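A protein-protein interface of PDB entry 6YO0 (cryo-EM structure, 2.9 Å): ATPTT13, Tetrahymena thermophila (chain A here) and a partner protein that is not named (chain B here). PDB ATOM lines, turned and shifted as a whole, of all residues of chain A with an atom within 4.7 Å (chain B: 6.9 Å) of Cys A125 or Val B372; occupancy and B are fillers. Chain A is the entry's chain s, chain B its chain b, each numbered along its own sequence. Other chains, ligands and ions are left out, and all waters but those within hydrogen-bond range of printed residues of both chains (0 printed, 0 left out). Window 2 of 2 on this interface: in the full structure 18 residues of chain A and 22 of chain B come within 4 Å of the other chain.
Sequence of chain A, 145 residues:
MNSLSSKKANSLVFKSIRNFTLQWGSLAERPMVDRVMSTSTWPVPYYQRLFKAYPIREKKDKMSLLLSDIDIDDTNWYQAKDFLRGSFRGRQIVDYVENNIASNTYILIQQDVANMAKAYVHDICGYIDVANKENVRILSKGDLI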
ATOM      1  N   VAL A 121      -2.455 -17.999 -30.629  1.00  0.00           N
ATOM      2  CA  VAL A 121      -1.168 -17.632 -30.047  1.00  0.00           C
ATOM      3  C   VAL A 121      -0.764 -16.233 -30.488  1.00  0.00           C
ATOM      4  O   VAL A 121      -0.360 -15.398 -29.671  1.00  0.00           O
ATOM      5  CB  VAL A 121      -0.097 -18.670 -30.427  1.00  0.00           C
ATOM      6  CG1 VAL A 121       1.287 -18.141 -30.127  1.00  0.00           C
ATOM      7  CG2 VAL A 121      -0.330 -19.969 -29.681  1.00  0.00           C
ATOM      8  N   HIS A 122      -0.869 -15.955 -31.786  1.00  0.00           N
ATOM      9  CA  HIS A 122      -0.505 -14.631 -32.279  1.00  0.00           C
ATOM     10  C   HIS A 122      -1.339 -13.543 -31.615  1.00  0.00           C
ATOM     11  O   HIS A 122      -0.804 -12.507 -31.202  1.00  0.00           O
ATOM     12  CB  HIS A 122      -0.658 -14.587 -33.797  1.00  0.00           C
ATOM     13  CG  HIS A 122       0.458 -15.263 -34.527  1.00  0.00           C
ATOM     14  ND1 HIS A 122       0.699 -16.615 -34.424  1.00  0.00           N
ATOM     15  CD2 HIS A 122       1.406 -14.774 -35.360  1.00  0.00           C
ATOM     16  CE1 HIS A 122       1.744 -16.932 -35.169  1.00  0.00           C
ATOM     17  NE2 HIS A 122       2.192 -15.833 -35.747  1.00  0.00           N
ATOM     18  N   ASP A 123      -2.651 -13.757 -31.504  1.00  0.00           N
ATOM     19  CA  ASP A 123      -3.511 -12.753 -30.884  1.00  0.00           C
ATOM     20  C   ASP A 123      -3.119 -12.511 -29.433  1.00  0.00           C
ATOM     21  O   ASP A 123      -2.915 -11.367 -29.013  1.00  0.00           O
ATOM     22  CB  ASP A 123      -4.971 -13.186 -30.971  1.00  0.00           C
ATOM     23  CG  ASP A 123      -5.894 -12.242 -30.236  1.00  0.00           C
ATOM     24  OD1 ASP A 123      -5.991 -11.070 -30.652  1.00  0.00           O
ATOM     25  OD2 ASP A 123      -6.511 -12.663 -29.236  1.00  0.00           O
ATOM     26  N   ILE A 124      -3.012 -13.586 -28.649  1.00  0.00           N
ATOM     27  CA  ILE A 124      -2.699 -13.443 -27.231  1.00  0.00           C
ATOM     28  C   ILE A 124      -1.345 -12.773 -27.056  1.00  0.00           C
ATOM     29  O   ILE A 124      -1.137 -11.991 -26.120  1.00  0.00           O
ATOM     30  CB  ILE A 124      -2.759 -14.809 -26.526  1.00  0.00           C
ATOM     31  CG1 ILE A 124      -4.159 -15.417 -26.638  1.00  0.00           C
ATOM     32  CG2 ILE A 124      -2.394 -14.665 -25.069  1.00  0.00           C
ATOM     33  CD1 ILE A 124      -5.262 -14.596 -25.991  1.00  0.00           C
ATOM     34  N   CYS A 125      -0.404 -13.062 -27.955  1.00  0.00           N
ATOM     35  CA  CYS A 125       0.912 -12.449 -27.843  1.00  0.00           C
ATOM     36  C   CYS A 125       0.848 -10.970 -28.188  1.00  0.00           C
ATOM     37  O   CYS A 125       1.628 -10.175 -27.655  1.00  0.00           O
ATOM     38  CB  CYS A 125       1.902 -13.165 -28.758  1.00  0.00           C
ATOM     39  SG  CYS A 125       3.587 -12.520 -28.676  1.00  0.00           S
ATOM     40  N   GLY A 126      -0.070 -10.586 -29.075  1.00  0.00           N
ATOM     41  CA  GLY A 126      -0.190  -9.187 -29.442  1.00  0.00           C
ATOM     42  C   GLY A 126      -0.422  -8.288 -28.243  1.00  0.00           C
ATOM     43  O   GLY A 126       0.062  -7.153 -28.212  1.00  0.00           O
ATOM     44  N   TYR A 127      -1.158  -8.777 -27.244  1.00  0.00           N
ATOM     45  CA  TYR A 127      -1.549  -7.981 -26.090  1.00  0.00           C
ATOM     46  C   TYR A 127      -0.589  -8.139 -24.917  1.00  0.00           C
ATOM     47  O   TYR A 127      -0.946  -7.797 -23.784  1.00  0.00           O
ATOM     48  CB  TYR A 127      -2.969  -8.352 -25.656  1.00  0.00           C
ATOM     49  CG  TYR A 127      -4.067  -7.836 -26.566  1.00  0.00           C
ATOM     50  CD1 TYR A 127      -5.341  -8.384 -26.520  1.00  0.00           C
ATOM     51  CD2 TYR A 127      -3.833  -6.805 -27.472  1.00  0.00           C
ATOM     52  CE1 TYR A 127      -6.350  -7.920 -27.347  1.00  0.00           C
ATOM     53  CE2 TYR A 127      -4.834  -6.337 -28.299  1.00  0.00           C
ATOM     54  CZ  TYR A 127      -6.089  -6.896 -28.233  1.00  0.00           C
ATOM     55  OH  TYR A 127      -7.085  -6.426 -29.060  1.00  0.00           O
ATOM     56  N   ILE A 128       0.612  -8.650 -25.162  1.00  0.00           N
ATOM     57  CA  ILE A 128       1.666  -8.682 -24.157  1.00  0.00           C
ATOM     58  C   ILE A 128       2.281  -7.289 -24.104  1.00  0.00           C
ATOM     59  O   ILE A 128       2.012  -6.455 -24.975  1.00  0.00           O
ATOM     60  CB  ILE A 128       2.712  -9.758 -24.496  1.00  0.00           C
ATOM     61  CG1 ILE A 128       3.654 -10.016 -23.320  1.00  0.00           C
ATOM     62  CG2 ILE A 128       3.533  -9.323 -25.693  1.00  0.00           C
ATOM     63  CD1 ILE A 128       4.701 -11.060 -23.620  1.00  0.00           C
ATOM     64  N   LEU B 362       9.948 -17.235 -21.956  1.00  0.00           N
ATOM     65  CA  LEU B 362       9.098 -18.298 -22.459  1.00  0.00           C
ATOM     66  C   LEU B 362       9.914 -19.221 -23.358  1.00  0.00           C
ATOM     67  O   LEU B 362      11.143 -19.128 -23.435  1.00  0.00           O
ATOM     68  CB  LEU B 362       7.902 -17.723 -23.216  1.00  0.00           C
ATOM     69  CG  LEU B 362       7.116 -16.617 -22.523  1.00  0.00           C
ATOM     70  CD1 LEU B 362       7.797 -15.282 -22.725  1.00  0.00           C
ATOM     71  CD2 LEU B 362       5.699 -16.578 -23.032  1.00  0.00           C
ATOM     72  N   LEU B 366      10.640 -20.763 -30.086  1.00  0.00           N
ATOM     73  CA  LEU B 366       9.264 -20.770 -30.557  1.00  0.00           C
ATOM     74  C   LEU B 366       8.683 -19.375 -30.686  1.00  0.00           C
ATOM     75  O   LEU B 366       7.762 -19.173 -31.479  1.00  0.00           O
ATOM     76  CB  LEU B 366       8.380 -21.605 -29.625  1.00  0.00           C
ATOM     77  CG  LEU B 366       8.883 -23.031 -29.394  1.00  0.00           C
ATOM     78  CD1 LEU B 366       7.949 -23.807 -28.478  1.00  0.00           C
ATOM     79  CD2 LEU B 366       9.050 -23.753 -30.718  1.00  0.00           C
ATOM     80  N   LYS B 367       9.205 -18.415 -29.926  1.00  0.00           N
ATOM     81  CA  LYS B 367       8.769 -17.024 -30.022  1.00  0.00           C
ATOM     82  C   LYS B 367       9.688 -16.265 -30.976  1.00  0.00           C
ATOM     83  O   LYS B 367      10.528 -15.449 -30.590  1.00  0.00           O
ATOM     84  CB  LYS B 367       8.748 -16.387 -28.640  1.00  0.00           C
ATOM     85  CG  LYS B 367       7.849 -17.091 -27.644  1.00  0.00           C
ATOM     86  CD  LYS B 367       6.424 -17.173 -28.152  1.00  0.00           C
ATOM     87  CE  LYS B 367       5.520 -17.886 -27.179  1.00  0.00           C
ATOM     88  NZ  LYS B 367       4.164 -18.047 -27.747  1.00  0.00           N
ATOM     89  N   ASN B 368       9.506 -16.561 -32.260  1.00  0.00           N
ATOM     90  CA  ASN B 368      10.267 -15.937 -33.329  1.00  0.00           C
ATOM     91  C   ASN B 368       9.401 -15.031 -34.187  1.00  0.00           C
ATOM     92  O   ASN B 368       9.886 -14.494 -35.190  1.00  0.00           O
ATOM     93  CB  ASN B 368      10.928 -17.009 -34.199  1.00  0.00           C
ATOM     94  CG  ASN B 368      11.741 -17.994 -33.385  1.00  0.00           C
ATOM     95  OD1 ASN B 368      12.589 -17.601 -32.584  1.00  0.00           O
ATOM     96  ND2 ASN B 368      11.481 -19.280 -33.581  1.00  0.00           N
ATOM     97  N   ILE B 369       8.130 -14.850 -33.822  1.00  0.00           N
ATOM     98  CA  ILE B 369       7.254 -13.975 -34.581  1.00  0.00           C
ATOM     99  C   ILE B 369       7.813 -12.560 -34.552  1.00  0.00           C
ATOM    100  O   ILE B 369       8.452 -12.134 -33.583  1.00  0.00           O
ATOM    101  CB  ILE B 369       5.820 -14.009 -34.024  1.00  0.00           C
ATOM    102  CG1 ILE B 369       5.302 -15.448 -33.949  1.00  0.00           C
ATOM    103  CG2 ILE B 369       4.897 -13.158 -34.879  1.00  0.00           C
ATOM    104  CD1 ILE B 369       5.409 -16.212 -35.252  1.00  0.00           C
ATOM    105  N   GLU B 370       7.579 -11.819 -35.632  1.00  0.00           N
ATOM    106  CA  GLU B 370       8.173 -10.494 -35.737  1.00  0.00           C
ATOM    107  C   GLU B 370       7.673  -9.589 -34.620  1.00  0.00           C
ATOM    108  O   GLU B 370       8.449  -8.826 -34.032  1.00  0.00           O
ATOM    109  CB  GLU B 370       7.859  -9.887 -37.102  1.00  0.00           C
ATOM    110  CG  GLU B 370       8.519 -10.614 -38.261  1.00  0.00           C
ATOM    111  CD  GLU B 370       8.132 -10.037 -39.607  1.00  0.00           C
ATOM    112  OE1 GLU B 370       7.210  -9.195 -39.652  1.00  0.00           O
ATOM    113  OE2 GLU B 370       8.749 -10.426 -40.621  1.00  0.00           O
ATOM    114  N   SER B 371       6.377  -9.662 -34.311  1.00  0.00           N
ATOM    115  CA  SER B 371       5.828  -8.838 -33.241  1.00  0.00           C
ATOM    116  C   SER B 371       6.463  -9.156 -31.892  1.00  0.00           C
ATOM    117  O   SER B 371       6.790  -8.241 -31.129  1.00  0.00           O
ATOM    118  CB  SER B 371       4.313  -9.026 -33.166  1.00  0.00           C
ATOM    119  OG  SER B 371       3.755  -8.233 -32.134  1.00  0.00           O
ATOM    120  N   VAL B 372       6.672 -10.438 -31.580  1.00  0.00           N
ATOM    121  CA  VAL B 372       7.257 -10.771 -30.282  1.00  0.00           C
ATOM    122  C   VAL B 372       8.673 -10.215 -30.183  1.00  0.00           C
ATOM    123  O   VAL B 372       9.033  -9.565 -29.195  1.00  0.00           O
ATOM    124  CB  VAL B 372       7.196 -12.289 -30.015  1.00  0.00           C
ATOM    125  CG1 VAL B 372       8.003 -13.104 -31.015  1.00  0.00           C
ATOM    126  CG2 VAL B 372       7.658 -12.585 -28.600  1.00  0.00           C
ATOM    127  N   LYS B 373       9.495 -10.439 -31.212  1.00  0.00           N
ATOM    128  CA  LYS B 373      10.869  -9.956 -31.155  1.00  0.00           C
ATOM    129  C   LYS B 373      10.902  -8.438 -31.111  1.00  0.00           C
ATOM    130  O   LYS B 373      11.768  -7.848 -30.454  1.00  0.00           O
ATOM    131  CB  LYS B 373      11.672 -10.463 -32.352  1.00  0.00           C
ATOM    132  CG  LYS B 373      11.504 -11.941 -32.644  1.00  0.00           C
ATOM    133  CD  LYS B 373      12.593 -12.453 -33.574  1.00  0.00           C
ATOM    134  CE  LYS B 373      13.955 -12.492 -32.893  1.00  0.00           C
ATOM    135  NZ  LYS B 373      15.003 -13.086 -33.766  1.00  0.00           N
ATOM    136  N   LYS B 374       9.963  -7.795 -31.800  1.00  0.00           N
ATOM    137  CA  LYS B 374       9.858  -6.343 -31.751  1.00  0.00           C
ATOM    138  C   LYS B 374       9.568  -5.872 -30.332  1.00  0.00           C
ATOM    139  O   LYS B 374      10.237  -4.971 -29.814  1.00  0.00           O
ATOM    140  CB  LYS B 374       8.764  -5.884 -32.713  1.00  0.00           C
ATOM    141  CG  LYS B 374       8.586  -4.386 -32.812  1.00  0.00           C
ATOM    142  CD  LYS B 374       7.331  -4.046 -33.595  1.00  0.00           C
ATOM    143  CE  LYS B 374       7.168  -2.548 -33.766  1.00  0.00           C
ATOM    144  NZ  LYS B 374       8.204  -1.985 -34.673  1.00  0.00           N
ATOM    145  N   ILE B 375       8.573  -6.481 -29.684  1.00  0.00           N
ATOM    146  CA  ILE B 375       8.233  -6.102 -28.316  1.00  0.00           C
ATOM    147  C   ILE B 375       9.423  -6.302 -27.387  1.00  0.00           C
ATOM    148  O   ILE B 375       9.691  -5.469 -26.514  1.00  0.00           O
ATOM    149  CB  ILE B 375       7.005  -6.898 -27.840  1.00  0.00           C
ATOM    150  CG1 ILE B 375       5.789  -6.569 -28.707  1.00  0.00           C
ATOM    151  CG2 ILE B 375       6.703  -6.599 -26.387  1.00  0.00           C
ATOM    152  CD1 ILE B 375       4.539  -7.348 -28.342  1.00  0.00           C
ATOM    153  N   LEU B 376      10.156  -7.403 -27.557  1.00  0.00           N
ATOM    154  CA  LEU B 376      11.307  -7.648 -26.693  1.00  0.00           C
ATOM    155  C   LEU B 376      12.385  -6.598 -26.916  1.00  0.00           C
ATOM    156  O   LEU B 376      12.956  -6.065 -25.958  1.00  0.00           O
ATOM    157  CB  LEU B 376      11.863  -9.050 -26.933  1.00  0.00           C
ATOM    158  CG  LEU B 376      10.904 -10.209 -26.659  1.00  0.00           C
ATOM    159  CD1 LEU B 376      11.591 -11.538 -26.902  1.00  0.00           C
ATOM    160  CD2 LEU B 376      10.373 -10.138 -25.243  1.00  0.00           C
ATOM    161  N   ALA B 377      12.680  -6.289 -28.178  1.00  0.00           N
ATOM    162  CA  ALA B 377      13.701  -5.290 -28.463  1.00  0.00           C
ATOM    163  C   ALA B 377      13.324  -3.941 -27.866  1.00  0.00           C
ATOM    164  O   ALA B 377      14.176  -3.239 -27.310  1.00  0.00           O
ATOM    165  CB  ALA B 377      13.907  -5.173 -29.972  1.00  0.00           C
ATOM    166  N   THR B 378      12.048  -3.564 -27.970  1.00  0.00           N
ATOM    167  CA  THR B 378      11.539  -2.333 -27.378  1.00  0.00           C
ATOM    168  C   THR B 378      10.963  -2.548 -25.985  1.00  0.00           C
ATOM    169  O   THR B 378      10.095  -1.778 -25.553  1.00  0.00           O
ATOM    170  CB  THR B 378      10.480  -1.712 -28.288  1.00  0.00           C
ATOM    171  OG1 THR B 378      10.047  -0.463 -27.736  1.00  0.00           O
ATOM    172  CG2 THR B 378       9.279  -2.637 -28.416  1.00  0.00           C
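Among the printed residues, pairs that only touch across the chains: His A122 with Ile B369, Ile A128 with Ile B375, Val A121 with Lys B367 and Cys A125 with Val B372.
Printed residues of chain B within 4 Å of Val A121: Lys B367 (3.7 Å).
Of the printed residues of chain B, His A122 touches Ile B369.
Printed residues of chain B within 4 Å of Ile A128: Ile B375 (3.5 Å).
Printed residues of chain A within 4 Å of Lys B367: Val A121 (3.7 Å).
Printed residues of chain A within 4 Å of Ile B369: His A122.
Val B372 touches just one residue of chain A: Cys A125.
The nearest printed residue of chain A that does not touch Val B372 is Ile A128 (6.0 Å).
The nearest printed residue of chain A that does not touch Lys B367 is Cys A125 (5.5 Å).
Of the 8 printed residues of chain A, 4 touch a printed residue of chain B.
Printed residues of chain B that touch a printed residue of chain A: Lys B367, Ile B369, Val B372 and Ile B375.
Along chain B the printed residues that touch a printed residue of chain A span positions 367 to 375.
Among the printed residues, 4 pairs touch across the chains.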
